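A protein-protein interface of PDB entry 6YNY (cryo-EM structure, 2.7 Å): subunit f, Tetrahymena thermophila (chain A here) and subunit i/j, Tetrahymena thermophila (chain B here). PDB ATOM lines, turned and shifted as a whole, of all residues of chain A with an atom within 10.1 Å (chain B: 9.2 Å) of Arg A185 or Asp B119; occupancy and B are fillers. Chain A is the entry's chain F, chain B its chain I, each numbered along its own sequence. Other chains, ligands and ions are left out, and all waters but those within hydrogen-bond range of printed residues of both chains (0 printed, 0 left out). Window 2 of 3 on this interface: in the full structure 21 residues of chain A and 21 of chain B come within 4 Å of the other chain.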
ATOM      1  N   GLY A 176      -6.857 -16.533  38.064  1.00  0.00           N
ATOM      2  CA  GLY A 176      -6.418 -16.368  36.692  1.00  0.00           C
ATOM      3  C   GLY A 176      -4.982 -15.908  36.565  1.00  0.00           C
ATOM      4  O   GLY A 176      -4.325 -16.184  35.560  1.00  0.00           O
ATOM      5  N   ASN A 177      -4.475 -15.199  37.573  1.00  0.00           N
ATOM      6  CA  ASN A 177      -3.107 -14.703  37.537  1.00  0.00           C
ATOM      7  C   ASN A 177      -2.076 -15.812  37.678  1.00  0.00           C
ATOM      8  O   ASN A 177      -0.883 -15.549  37.501  1.00  0.00           O
ATOM      9  CB  ASN A 177      -2.912 -13.656  38.633  1.00  0.00           C
ATOM     10  CG  ASN A 177      -1.611 -12.905  38.496  1.00  0.00           C
ATOM     11  OD1 ASN A 177      -1.435 -12.113  37.573  1.00  0.00           O
ATOM     12  ND2 ASN A 177      -0.699 -13.126  39.430  1.00  0.00           N
ATOM     13  N   SER A 178      -2.502 -17.031  37.991  1.00  0.00           N
ATOM     14  CA  SER A 178      -1.604 -18.169  38.093  1.00  0.00           C
ATOM     15  C   SER A 178      -1.447 -18.923  36.782  1.00  0.00           C
ATOM     16  O   SER A 178      -0.589 -19.807  36.695  1.00  0.00           O
ATOM     17  CB  SER A 178      -2.100 -19.126  39.176  1.00  0.00           C
ATOM     18  OG  SER A 178      -2.088 -18.499  40.444  1.00  0.00           O
ATOM     19  N   ILE A 179      -2.251 -18.608  35.773  1.00  0.00           N
ATOM     20  CA  ILE A 179      -2.108 -19.189  34.445  1.00  0.00           C
ATOM     21  C   ILE A 179      -1.119 -18.330  33.671  1.00  0.00           C
ATOM     22  O   ILE A 179      -1.363 -17.141  33.440  1.00  0.00           O
ATOM     23  CB  ILE A 179      -3.461 -19.272  33.724  1.00  0.00           C
ATOM     24  CG1 ILE A 179      -4.409 -20.188  34.493  1.00  0.00           C
ATOM     25  CG2 ILE A 179      -3.276 -19.786  32.319  1.00  0.00           C
ATOM     26  CD1 ILE A 179      -5.847 -20.083  34.069  1.00  0.00           C
ATOM     27  N   VAL A 180      -0.001 -18.931  33.270  1.00  0.00           N
ATOM     28  CA  VAL A 180       1.159 -18.185  32.813  1.00  0.00           C
ATOM     29  C   VAL A 180       1.627 -18.700  31.461  1.00  0.00           C
ATOM     30  O   VAL A 180       1.261 -19.789  31.015  1.00  0.00           O
ATOM     31  CB  VAL A 180       2.314 -18.267  33.829  1.00  0.00           C
ATOM     32  CG1 VAL A 180       1.846 -17.821  35.185  1.00  0.00           C
ATOM     33  CG2 VAL A 180       2.849 -19.675  33.902  1.00  0.00           C
ATOM     34  N   VAL A 181       2.447 -17.885  30.812  1.00  0.00           N
ATOM     35  CA  VAL A 181       3.189 -18.304  29.632  1.00  0.00           C
ATOM     36  C   VAL A 181       4.342 -19.190  30.073  1.00  0.00           C
ATOM     37  O   VAL A 181       4.999 -18.920  31.084  1.00  0.00           O
ATOM     38  CB  VAL A 181       3.694 -17.077  28.852  1.00  0.00           C
ATOM     39  CG1 VAL A 181       4.597 -17.497  27.726  1.00  0.00           C
ATOM     40  CG2 VAL A 181       2.534 -16.268  28.322  1.00  0.00           C
ATOM     41  N   ASN A 182       4.592 -20.253  29.322  1.00  0.00           N
ATOM     42  CA  ASN A 182       5.651 -21.177  29.687  1.00  0.00           C
ATOM     43  C   ASN A 182       7.000 -20.464  29.654  1.00  0.00           C
ATOM     44  O   ASN A 182       7.284 -19.732  28.698  1.00  0.00           O
ATOM     45  CB  ASN A 182       5.670 -22.370  28.739  1.00  0.00           C
ATOM     46  CG  ASN A 182       6.581 -23.470  29.217  1.00  0.00           C
ATOM     47  OD1 ASN A 182       7.799 -23.374  29.108  1.00  0.00           O
ATOM     48  ND2 ASN A 182       5.994 -24.527  29.745  1.00  0.00           N
ATOM     49  N   PRO A 183       7.858 -20.648  30.664  1.00  0.00           N
ATOM     50  CA  PRO A 183       9.158 -19.960  30.658  1.00  0.00           C
ATOM     51  C   PRO A 183      10.083 -20.399  29.540  1.00  0.00           C
ATOM     52  O   PRO A 183      11.095 -19.729  29.308  1.00  0.00           O
ATOM     53  CB  PRO A 183       9.747 -20.307  32.028  1.00  0.00           C
ATOM     54  CG  PRO A 183       8.618 -20.768  32.836  1.00  0.00           C
ATOM     55  CD  PRO A 183       7.663 -21.410  31.906  1.00  0.00           C
ATOM     56  N   CYS A 184       9.784 -21.503  28.854  1.00  0.00           N
ATOM     57  CA  CYS A 184      10.567 -21.883  27.687  1.00  0.00           C
ATOM     58  C   CYS A 184      10.628 -20.761  26.665  1.00  0.00           C
ATOM     59  O   CYS A 184      11.563 -20.715  25.859  1.00  0.00           O
ATOM     60  CB  CYS A 184       9.978 -23.136  27.046  1.00  0.00           C
ATOM     61  SG  CYS A 184      10.279 -24.667  27.947  1.00  0.00           S
ATOM     62  N   ARG A 185       9.651 -19.856  26.685  1.00  0.00           N
ATOM     63  CA  ARG A 185       9.692 -18.681  25.827  1.00  0.00           C
ATOM     64  C   ARG A 185      11.003 -17.928  25.987  1.00  0.00           C
ATOM     65  O   ARG A 185      11.544 -17.389  25.014  1.00  0.00           O
ATOM     66  CB  ARG A 185       8.500 -17.781  26.157  1.00  0.00           C
ATOM     67  CG  ARG A 185       8.420 -16.464  25.404  1.00  0.00           C
ATOM     68  CD  ARG A 185       9.268 -15.354  26.013  1.00  0.00           C
ATOM     69  NE  ARG A 185       9.197 -15.302  27.468  1.00  0.00           N
ATOM     70  CZ  ARG A 185       8.195 -14.768  28.153  1.00  0.00           C
ATOM     71  NH1 ARG A 185       7.163 -14.235  27.522  1.00  0.00           N
ATOM     72  NH2 ARG A 185       8.226 -14.768  29.474  1.00  0.00           N
ATOM     73  N   ASN A 186      11.535 -17.882  27.207  1.00  0.00           N
ATOM     74  CA  ASN A 186      12.760 -17.138  27.459  1.00  0.00           C
ATOM     75  C   ASN A 186      13.975 -17.768  26.798  1.00  0.00           C
ATOM     76  O   ASN A 186      15.005 -17.102  26.667  1.00  0.00           O
ATOM     77  CB  ASN A 186      12.992 -17.016  28.960  1.00  0.00           C
ATOM     78  CG  ASN A 186      11.938 -16.184  29.642  1.00  0.00           C
ATOM     79  OD1 ASN A 186      11.299 -15.338  29.020  1.00  0.00           O
ATOM     80  ND2 ASN A 186      11.752 -16.414  30.928  1.00  0.00           N
ATOM     81  N   GLN A 187      13.884 -19.027  26.381  1.00  0.00           N
ATOM     82  CA  GLN A 187      15.002 -19.677  25.716  1.00  0.00           C
ATOM     83  C   GLN A 187      15.182 -19.214  24.280  1.00  0.00           C
ATOM     84  O   GLN A 187      16.216 -19.515  23.675  1.00  0.00           O
ATOM     85  CB  GLN A 187      14.818 -21.190  25.751  1.00  0.00           C
ATOM     86  CG  GLN A 187      14.573 -21.737  27.134  1.00  0.00           C
ATOM     87  CD  GLN A 187      15.643 -21.330  28.118  1.00  0.00           C
ATOM     88  OE1 GLN A 187      16.817 -21.218  27.769  1.00  0.00           O
ATOM     89  NE2 GLN A 187      15.241 -21.093  29.354  1.00  0.00           N
ATOM     90  N   ASN A 188      14.209 -18.501  23.719  1.00  0.00           N
ATOM     91  CA  ASN A 188      14.369 -17.924  22.395  1.00  0.00           C
ATOM     92  C   ASN A 188      15.312 -16.733  22.397  1.00  0.00           C
ATOM     93  O   ASN A 188      15.751 -16.309  21.325  1.00  0.00           O
ATOM     94  CB  ASN A 188      13.011 -17.512  21.841  1.00  0.00           C
ATOM     95  CG  ASN A 188      12.056 -18.671  21.731  1.00  0.00           C
ATOM     96  OD1 ASN A 188      12.468 -19.818  21.575  1.00  0.00           O
ATOM     97  ND2 ASN A 188      10.772 -18.380  21.812  1.00  0.00           N
ATOM     98  N   TYR A 189      15.621 -16.182  23.571  1.00  0.00           N
ATOM     99  CA  TYR A 189      16.602 -15.113  23.665  1.00  0.00           C
ATOM    100  C   TYR A 189      18.006 -15.600  23.351  1.00  0.00           C
ATOM    101  O   TYR A 189      18.887 -14.781  23.079  1.00  0.00           O
ATOM    102  CB  TYR A 189      16.559 -14.494  25.059  1.00  0.00           C
ATOM    103  CG  TYR A 189      15.381 -13.584  25.278  1.00  0.00           C
ATOM    104  CD1 TYR A 189      14.134 -14.094  25.583  1.00  0.00           C
ATOM    105  CD2 TYR A 189      15.517 -12.213  25.176  1.00  0.00           C
ATOM    106  CE1 TYR A 189      13.059 -13.267  25.778  1.00  0.00           C
ATOM    107  CE2 TYR A 189      14.449 -11.376  25.369  1.00  0.00           C
ATOM    108  CZ  TYR A 189      13.220 -11.905  25.671  1.00  0.00           C
ATOM    109  OH  TYR A 189      12.149 -11.068  25.865  1.00  0.00           O
ATOM    110  N   ARG A 190      18.231 -16.912  23.386  1.00  0.00           N
ATOM    111  CA  ARG A 190      19.524 -17.452  22.989  1.00  0.00           C
ATOM    112  C   ARG A 190      19.852 -17.084  21.550  1.00  0.00           C
ATOM    113  O   ARG A 190      21.016 -16.842  21.212  1.00  0.00           O
ATOM    114  CB  ARG A 190      19.525 -18.966  23.165  1.00  0.00           C
ATOM    115  CG  ARG A 190      19.162 -19.429  24.556  1.00  0.00           C
ATOM    116  CD  ARG A 190      19.162 -20.934  24.653  1.00  0.00           C
ATOM    117  NE  ARG A 190      18.838 -21.403  25.992  1.00  0.00           N
ATOM    118  CZ  ARG A 190      19.102 -22.625  26.437  1.00  0.00           C
ATOM    119  NH1 ARG A 190      19.706 -23.505  25.659  1.00  0.00           N
ATOM    120  NH2 ARG A 190      18.770 -22.964  27.668  1.00  0.00           N
ATOM    121  N   LEU A 191      18.837 -17.038  20.688  1.00  0.00           N
ATOM    122  CA  LEU A 191      19.048 -16.603  19.313  1.00  0.00           C
ATOM    123  C   LEU A 191      19.624 -15.197  19.261  1.00  0.00           C
ATOM    124  O   LEU A 191      20.481 -14.899  18.421  1.00  0.00           O
ATOM    125  CB  LEU A 191      17.731 -16.656  18.548  1.00  0.00           C
ATOM    126  CG  LEU A 191      17.079 -18.024  18.406  1.00  0.00           C
ATOM    127  CD1 LEU A 191      15.630 -17.873  18.015  1.00  0.00           C
ATOM    128  CD2 LEU A 191      17.814 -18.836  17.377  1.00  0.00           C
ATOM    129  N   TYR A 192      19.162 -14.317  20.146  1.00  0.00           N
ATOM    130  CA  TYR A 192      19.634 -12.939  20.128  1.00  0.00           C
ATOM    131  C   TYR A 192      21.094 -12.853  20.545  1.00  0.00           C
ATOM    132  O   TYR A 192      21.877 -12.115  19.938  1.00  0.00           O
ATOM    133  CB  TYR A 192      18.765 -12.080  21.044  1.00  0.00           C
ATOM    134  CG  TYR A 192      17.282 -12.191  20.785  1.00  0.00           C
ATOM    135  CD1 TYR A 192      16.363 -11.857  21.763  1.00  0.00           C
ATOM    136  CD2 TYR A 192      16.801 -12.627  19.565  1.00  0.00           C
ATOM    137  CE1 TYR A 192      15.014 -11.955  21.533  1.00  0.00           C
ATOM    138  CE2 TYR A 192      15.453 -12.730  19.328  1.00  0.00           C
ATOM    139  CZ  TYR A 192      14.564 -12.393  20.314  1.00  0.00           C
ATOM    140  OH  TYR A 192      13.217 -12.492  20.076  1.00  0.00           O
ATOM    141  N   PHE A 193      21.478 -13.598  21.579  1.00  0.00           N
ATOM    142  CA  PHE A 193      22.858 -13.573  22.040  1.00  0.00           C
ATOM    143  C   PHE A 193      23.808 -14.136  20.996  1.00  0.00           C
ATOM    144  O   PHE A 193      24.957 -13.692  20.903  1.00  0.00           O
ATOM    145  CB  PHE A 193      22.976 -14.353  23.347  1.00  0.00           C
ATOM    146  CG  PHE A 193      22.041 -13.882  24.415  1.00  0.00           C
ATOM    147  CD1 PHE A 193      21.779 -12.538  24.580  1.00  0.00           C
ATOM    148  CD2 PHE A 193      21.411 -14.783  25.245  1.00  0.00           C
ATOM    149  CE1 PHE A 193      20.920 -12.107  25.554  1.00  0.00           C
ATOM    150  CE2 PHE A 193      20.548 -14.353  26.222  1.00  0.00           C
ATOM    151  CZ  PHE A 193      20.303 -13.014  26.376  1.00  0.00           C
ATOM    152  N   ASP B 112      -1.508  -7.194  38.739  1.00  0.00           N
ATOM    153  CA  ASP B 112      -0.667  -6.580  37.717  1.00  0.00           C
ATOM    154  C   ASP B 112       0.577  -5.931  38.303  1.00  0.00           C
ATOM    155  O   ASP B 112       1.603  -5.835  37.620  1.00  0.00           O
ATOM    156  CB  ASP B 112      -1.475  -5.545  36.938  1.00  0.00           C
ATOM    157  CG  ASP B 112      -2.727  -6.126  36.322  1.00  0.00           C
ATOM    158  OD1 ASP B 112      -2.946  -7.347  36.454  1.00  0.00           O
ATOM    159  OD2 ASP B 112      -3.497  -5.358  35.708  1.00  0.00           O
ATOM    160  N   CYS B 115       3.787  -8.642  39.233  1.00  0.00           N
ATOM    161  CA  CYS B 115       4.456  -9.454  38.227  1.00  0.00           C
ATOM    162  C   CYS B 115       4.381  -8.739  36.886  1.00  0.00           C
ATOM    163  O   CYS B 115       3.905  -7.604  36.789  1.00  0.00           O
ATOM    164  CB  CYS B 115       3.825 -10.845  38.142  1.00  0.00           C
ATOM    165  SG  CYS B 115       2.209 -10.886  37.339  1.00  0.00           S
ATOM    166  N   TYR B 116       4.862  -9.417  35.849  1.00  0.00           N
ATOM    167  CA  TYR B 116       4.787  -8.937  34.473  1.00  0.00           C
ATOM    168  C   TYR B 116       3.468  -9.428  33.894  1.00  0.00           C
ATOM    169  O   TYR B 116       3.349 -10.579  33.472  1.00  0.00           O
ATOM    170  CB  TYR B 116       5.989  -9.429  33.679  1.00  0.00           C
ATOM    171  CG  TYR B 116       6.043  -8.957  32.254  1.00  0.00           C
ATOM    172  CD1 TYR B 116       6.222  -7.620  31.954  1.00  0.00           C
ATOM    173  CD2 TYR B 116       5.942  -9.853  31.208  1.00  0.00           C
ATOM    174  CE1 TYR B 116       6.278  -7.188  30.650  1.00  0.00           C
ATOM    175  CE2 TYR B 116       5.999  -9.433  29.907  1.00  0.00           C
ATOM    176  CZ  TYR B 116       6.168  -8.103  29.631  1.00  0.00           C
ATOM    177  OH  TYR B 116       6.224  -7.696  28.324  1.00  0.00           O
ATOM    178  N   SER B 117       2.471  -8.548  33.885  1.00  0.00           N
ATOM    179  CA  SER B 117       1.121  -8.964  33.533  1.00  0.00           C
ATOM    180  C   SER B 117       0.992  -9.534  32.123  1.00  0.00           C
ATOM    181  O   SER B 117       0.171 -10.449  31.944  1.00  0.00           O
ATOM    182  CB  SER B 117       0.167  -7.777  33.728  1.00  0.00           C
ATOM    183  OG  SER B 117       0.530  -6.676  32.920  1.00  0.00           O
ATOM    184  N   PRO B 118       1.724  -9.067  31.110  1.00  0.00           N
ATOM    185  CA  PRO B 118       1.558  -9.645  29.768  1.00  0.00           C
ATOM    186  C   PRO B 118       1.841 -11.132  29.694  1.00  0.00           C
ATOM    187  O   PRO B 118       1.442 -11.771  28.714  1.00  0.00           O
ATOM    188  CB  PRO B 118       2.545  -8.839  28.918  1.00  0.00           C
ATOM    189  CG  PRO B 118       2.713  -7.578  29.645  1.00  0.00           C
ATOM    190  CD  PRO B 118       2.654  -7.930  31.086  1.00  0.00           C
ATOM    191  N   ASP B 119       2.516 -11.704  30.685  1.00  0.00           N
ATOM    192  CA  ASP B 119       2.725 -13.142  30.755  1.00  0.00           C
ATOM    193  C   ASP B 119       1.632 -13.854  31.536  1.00  0.00           C
ATOM    194  O   ASP B 119       1.748 -15.056  31.785  1.00  0.00           O
ATOM    195  CB  ASP B 119       4.083 -13.446  31.383  1.00  0.00           C
ATOM    196  CG  ASP B 119       5.236 -13.157  30.448  1.00  0.00           C
ATOM    197  OD1 ASP B 119       4.986 -12.711  29.310  1.00  0.00           O
ATOM    198  OD2 ASP B 119       6.396 -13.382  30.851  1.00  0.00           O
ATOM    199  N   ARG B 120       0.581 -13.143  31.924  1.00  0.00           N
ATOM    200  CA  ARG B 120      -0.530 -13.712  32.664  1.00  0.00           C
ATOM    201  C   ARG B 120      -1.808 -13.696  31.835  1.00  0.00           C
ATOM    202  O   ARG B 120      -1.996 -12.852  30.956  1.00  0.00           O
ATOM    203  CB  ARG B 120      -0.762 -12.958  33.973  1.00  0.00           C
ATOM    204  CG  ARG B 120       0.406 -12.985  34.928  1.00  0.00           C
ATOM    205  CD  ARG B 120       0.829 -14.394  35.214  1.00  0.00           C
ATOM    206  NE  ARG B 120       1.527 -14.530  36.485  1.00  0.00           N
ATOM    207  CZ  ARG B 120       2.791 -14.191  36.683  1.00  0.00           C
ATOM    208  NH1 ARG B 120       3.508 -13.674  35.698  1.00  0.00           N
ATOM    209  NH2 ARG B 120       3.329 -14.366  37.875  1.00  0.00           N
ATOM    210  N   PHE B 121      -2.684 -14.647  32.145  1.00  0.00           N
ATOM    211  CA  PHE B 121      -3.910 -14.835  31.376  1.00  0.00           C
ATOM    212  C   PHE B 121      -4.853 -13.639  31.432  1.00  0.00           C
ATOM    213  O   PHE B 121      -5.443 -13.307  30.388  1.00  0.00           O
ATOM    214  CB  PHE B 121      -4.606 -16.107  31.869  1.00  0.00           C
ATOM    215  CG  PHE B 121      -5.951 -16.342  31.267  1.00  0.00           C
ATOM    216  CD1 PHE B 121      -6.075 -16.846  29.990  1.00  0.00           C
ATOM    217  CD2 PHE B 121      -7.096 -16.072  31.985  1.00  0.00           C
ATOM    218  CE1 PHE B 121      -7.310 -17.062  29.444  1.00  0.00           C
ATOM    219  CE2 PHE B 121      -8.332 -16.289  31.439  1.00  0.00           C
ATOM    220  CZ  PHE B 121      -8.438 -16.785  30.168  1.00  0.00           C
ATOM    221  N   PRO B 122      -5.056 -12.972  32.570  1.00  0.00           N
ATOM    222  CA  PRO B 122      -5.998 -11.842  32.602  1.00  0.00           C
ATOM    223  C   PRO B 122      -5.648 -10.716  31.653  1.00  0.00           C
ATOM    224  O   PRO B 122      -6.541  -9.948  31.277  1.00  0.00           O
ATOM    225  CB  PRO B 122      -5.933 -11.379  34.061  1.00  0.00           C
ATOM    226  CG  PRO B 122      -5.445 -12.541  34.804  1.00  0.00           C
ATOM    227  CD  PRO B 122      -4.504 -13.245  33.902  1.00  0.00           C
ATOM    228  N   TYR B 123      -4.385 -10.582  31.254  1.00  0.00           N
ATOM    229  CA  TYR B 123      -4.023  -9.530  30.313  1.00  0.00           C
ATOM    230  C   TYR B 123      -4.634  -9.787  28.943  1.00  0.00           C
ATOM    231  O   TYR B 123      -5.079  -8.852  28.270  1.00  0.00           O
ATOM    232  CB  TYR B 123      -2.502  -9.429  30.216  1.00  0.00           C
ATOM    233  CG  TYR B 123      -1.991  -8.322  29.333  1.00  0.00           C
ATOM    234  CD1 TYR B 123      -1.971  -7.012  29.774  1.00  0.00           C
ATOM    235  CD2 TYR B 123      -1.509  -8.589  28.064  1.00  0.00           C
ATOM    236  CE1 TYR B 123      -1.500  -6.002  28.978  1.00  0.00           C
ATOM    237  CE2 TYR B 123      -1.036  -7.583  27.260  1.00  0.00           C
ATOM    238  CZ  TYR B 123      -1.032  -6.292  27.722  1.00  0.00           C
ATOM    239  OH  TYR B 123      -0.560  -5.284  26.921  1.00  0.00           O
ATOM    240  N   LEU B 124      -4.674 -11.048  28.520  1.00  0.00           N
ATOM    241  CA  LEU B 124      -5.262 -11.382  27.229  1.00  0.00           C
ATOM    242  C   LEU B 124      -6.729 -10.990  27.172  1.00  0.00           C
ATOM    243  O   LEU B 124      -7.218 -10.527  26.135  1.00  0.00           O
ATOM    244  CB  LEU B 124      -5.100 -12.874  26.960  1.00  0.00           C
ATOM    245  CG  LEU B 124      -4.103 -13.305  25.896  1.00  0.00           C
ATOM    246  CD1 LEU B 124      -2.779 -12.628  26.082  1.00  0.00           C
ATOM    247  CD2 LEU B 124      -3.946 -14.794  25.973  1.00  0.00           C
ATOM    248  N   LEU B 138      -2.802 -18.554  26.156  1.00  0.00           N
ATOM    249  CA  LEU B 138      -1.420 -18.093  26.184  1.00  0.00           C
ATOM    250  C   LEU B 138      -0.480 -19.023  25.431  1.00  0.00           C
ATOM    251  O   LEU B 138       0.634 -18.613  25.093  1.00  0.00           O
ATOM    252  CB  LEU B 138      -0.945 -17.941  27.624  1.00  0.00           C
ATOM    253  CG  LEU B 138      -1.524 -16.785  28.434  1.00  0.00           C
ATOM    254  CD1 LEU B 138      -1.105 -16.912  29.869  1.00  0.00           C
ATOM    255  CD2 LEU B 138      -1.080 -15.453  27.881  1.00  0.00           C
ATOM    256  N   ASN B 139      -0.899 -20.256  25.161  1.00  0.00           N
ATOM    257  CA  ASN B 139      -0.079 -21.226  24.446  1.00  0.00           C
ATOM    258  C   ASN B 139      -0.368 -21.260  22.955  1.00  0.00           C
ATOM    259  O   ASN B 139       0.560 -21.399  22.155  1.00  0.00           O
ATOM    260  CB  ASN B 139      -0.286 -22.623  25.028  1.00  0.00           C
ATOM    261  CG  ASN B 139       0.114 -22.713  26.476  1.00  0.00           C
ATOM    262  OD1 ASN B 139       0.954 -21.951  26.951  1.00  0.00           O
ATOM    263  ND2 ASN B 139      -0.480 -23.654  27.187  1.00  0.00           N
ATOM    264  N   ARG B 141      -0.367 -19.674  20.101  1.00  0.00           N
ATOM    265  CA  ARG B 141       0.138 -18.403  19.619  1.00  0.00           C
ATOM    266  C   ARG B 141       1.050 -18.611  18.424  1.00  0.00           C
ATOM    267  O   ARG B 141       1.832 -19.564  18.382  1.00  0.00           O
ATOM    268  CB  ARG B 141       0.893 -17.660  20.727  1.00  0.00           C
ATOM    269  CG  ARG B 141       2.093 -18.387  21.275  1.00  0.00           C
ATOM    270  CD  ARG B 141       2.789 -17.554  22.331  1.00  0.00           C
ATOM    271  NE  ARG B 141       4.027 -18.168  22.800  1.00  0.00           N
ATOM    272  CZ  ARG B 141       4.117 -18.993  23.838  1.00  0.00           C
ATOM    273  NH1 ARG B 141       5.293 -19.492  24.174  1.00  0.00           N
ATOM    274  NH2 ARG B 141       3.043 -19.317  24.539  1.00  0.00           N
ATOM    275  N   ALA B 144       5.819 -14.358  17.118  1.00  0.00           N
ATOM    276  CA  ALA B 144       5.969 -12.931  16.884  1.00  0.00           C
ATOM    277  C   ALA B 144       7.121 -12.636  15.937  1.00  0.00           C
ATOM    278  O   ALA B 144       7.120 -11.589  15.283  1.00  0.00           O
ATOM    279  CB  ALA B 144       6.184 -12.201  18.206  1.00  0.00           C
ATOM    280  N   HIS B 145       8.106 -13.530  15.858  1.00  0.00           N
ATOM    281  CA  HIS B 145       9.192 -13.358  14.904  1.00  0.00           C
ATOM    282  C   HIS B 145       8.663 -13.378  13.478  1.00  0.00           C
ATOM    283  O   HIS B 145       9.005 -12.518  12.660  1.00  0.00           O
ATOM    284  CB  HIS B 145      10.234 -14.456  15.097  1.00  0.00           C
ATOM    285  CG  HIS B 145      11.007 -14.350  16.372  1.00  0.00           C
ATOM    286  ND1 HIS B 145      11.705 -15.412  16.903  1.00  0.00           N
ATOM    287  CD2 HIS B 145      11.204 -13.311  17.216  1.00  0.00           C
ATOM    288  CE1 HIS B 145      12.292 -15.034  18.023  1.00  0.00           C
ATOM    289  NE2 HIS B 145      12.005 -13.763  18.235  1.00  0.00           N
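O of Asn A177 lies within hydrogen-bond range of NE of Arg B120 (2.8 Å). O of Ile A179 sits at hydrogen-bond distance from N of Phe B121 (3.1 Å). The backbone carbonyl oxygen (O) of Asp B119 is in hydrogen-bond range of the backbone NH (N) of Val A181. NH2 of Arg A185 is in salt-bridge range of OD2 of Asp B119, at 2.7 Å. NE2 of His B145 is in hydrogen-bond range of OH of Tyr A192, at 2.5 Å.
The side-chain amide oxygen (OD1) of Asn A186 is in hydrogen-bond range of the guanidinium group (NE) of Arg A185, at 2.6 Å. The side-chain amide nitrogen (ND2) of Asn A188 lies within hydrogen-bond range of the backbone carbonyl oxygen (O) of Arg A185, at 3.4 Å. NH1 of Arg B120 lies close to SG of Cys B115, at 3.5 Å. The guanidinium group (NH2) of Arg B141 lies within hydrogen-bond range of the backbone carbonyl oxygen (O) of Leu B138 (2.6 Å).
CB of Phe B121 touches O of Gly A176, at 3.7 Å. Gly A176 touches Pro B122 (O to CD, 3.4 Å). Cys B115 touches Asn A177 (SG to OD1, 3.9 Å). N of Asn A177 touches CG of Pro B122 (3.96 Å). O of Ile A179 touches CA of Arg B120 (3.6 Å). O of Ile A179 touches CD1 of Leu B138, at 3.6 Å. CA of Val A180 touches O of Asp B119, at 3.3 Å. CG1 of Val A180 touches NE of Arg B120, 3.6 Å away. C of Val A180 touches CD1 of Leu B138, 3.6 Å away. NH2 of Arg B141 touches CG1 of Val A181 (3.99 Å).
Of the printed residues of chain B, Arg A185 touches Asp B119 (2.7 Å). Asp B119 touches just these residues of chain A: Val A180 (3.3 Å), Val A181 (3.1 Å) and Arg A185 (2.7 Å). No residue of chain B comes within 4 Å of Cys A184. No residue of chain B comes within 4 Å of Asn A186. No residue of chain A comes within 4 Å of Ser B117. Of the printed residues of chain A, Arg B120 touches Asn A177 (2.8 Å), Ile A179 (3.6 Å) and Val A180 (3.6 Å). Of the printed residues of chain B, Gly A176 touches Phe B121 and Pro B122. Printed residues of chain B within 4 Å of Asn A177: Cys B115 (3.9 Å), Arg B120 (2.8 Å) and Pro B122 (3.96 Å). Printed residues of chain B within 4 Å of Val A181: Asp B119, Leu B138 and Arg B141. Phe A193 touches none of the printed residues of chain B.
Of the 16 printed residues of chain B, 8 touch a printed residue of chain A. Printed residues of chain B that touch a printed residue of chain A: Cys B115, Asp B119, Arg B120, Phe B121, Pro B122, Leu B138, Arg B141 and His B145. Hydrophobic or aromatic side chains of chain B within 4 Å of the printed part of chain A: Phe B121, Pro B122, Leu B138 and His B145. Along chain B the printed residues that touch a printed residue of chain A span positions 115 to 145. Hydrophobic or aromatic side chains of chain A within 4 Å of the printed part of chain B: Ile A179, Val A180, Val A181 and Tyr A192. Among the printed residues, Asp or Glu carboxylates within 4 Å of a Lys or Arg side-chain nitrogen of the other chain: Arg A185 with Asp B119.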
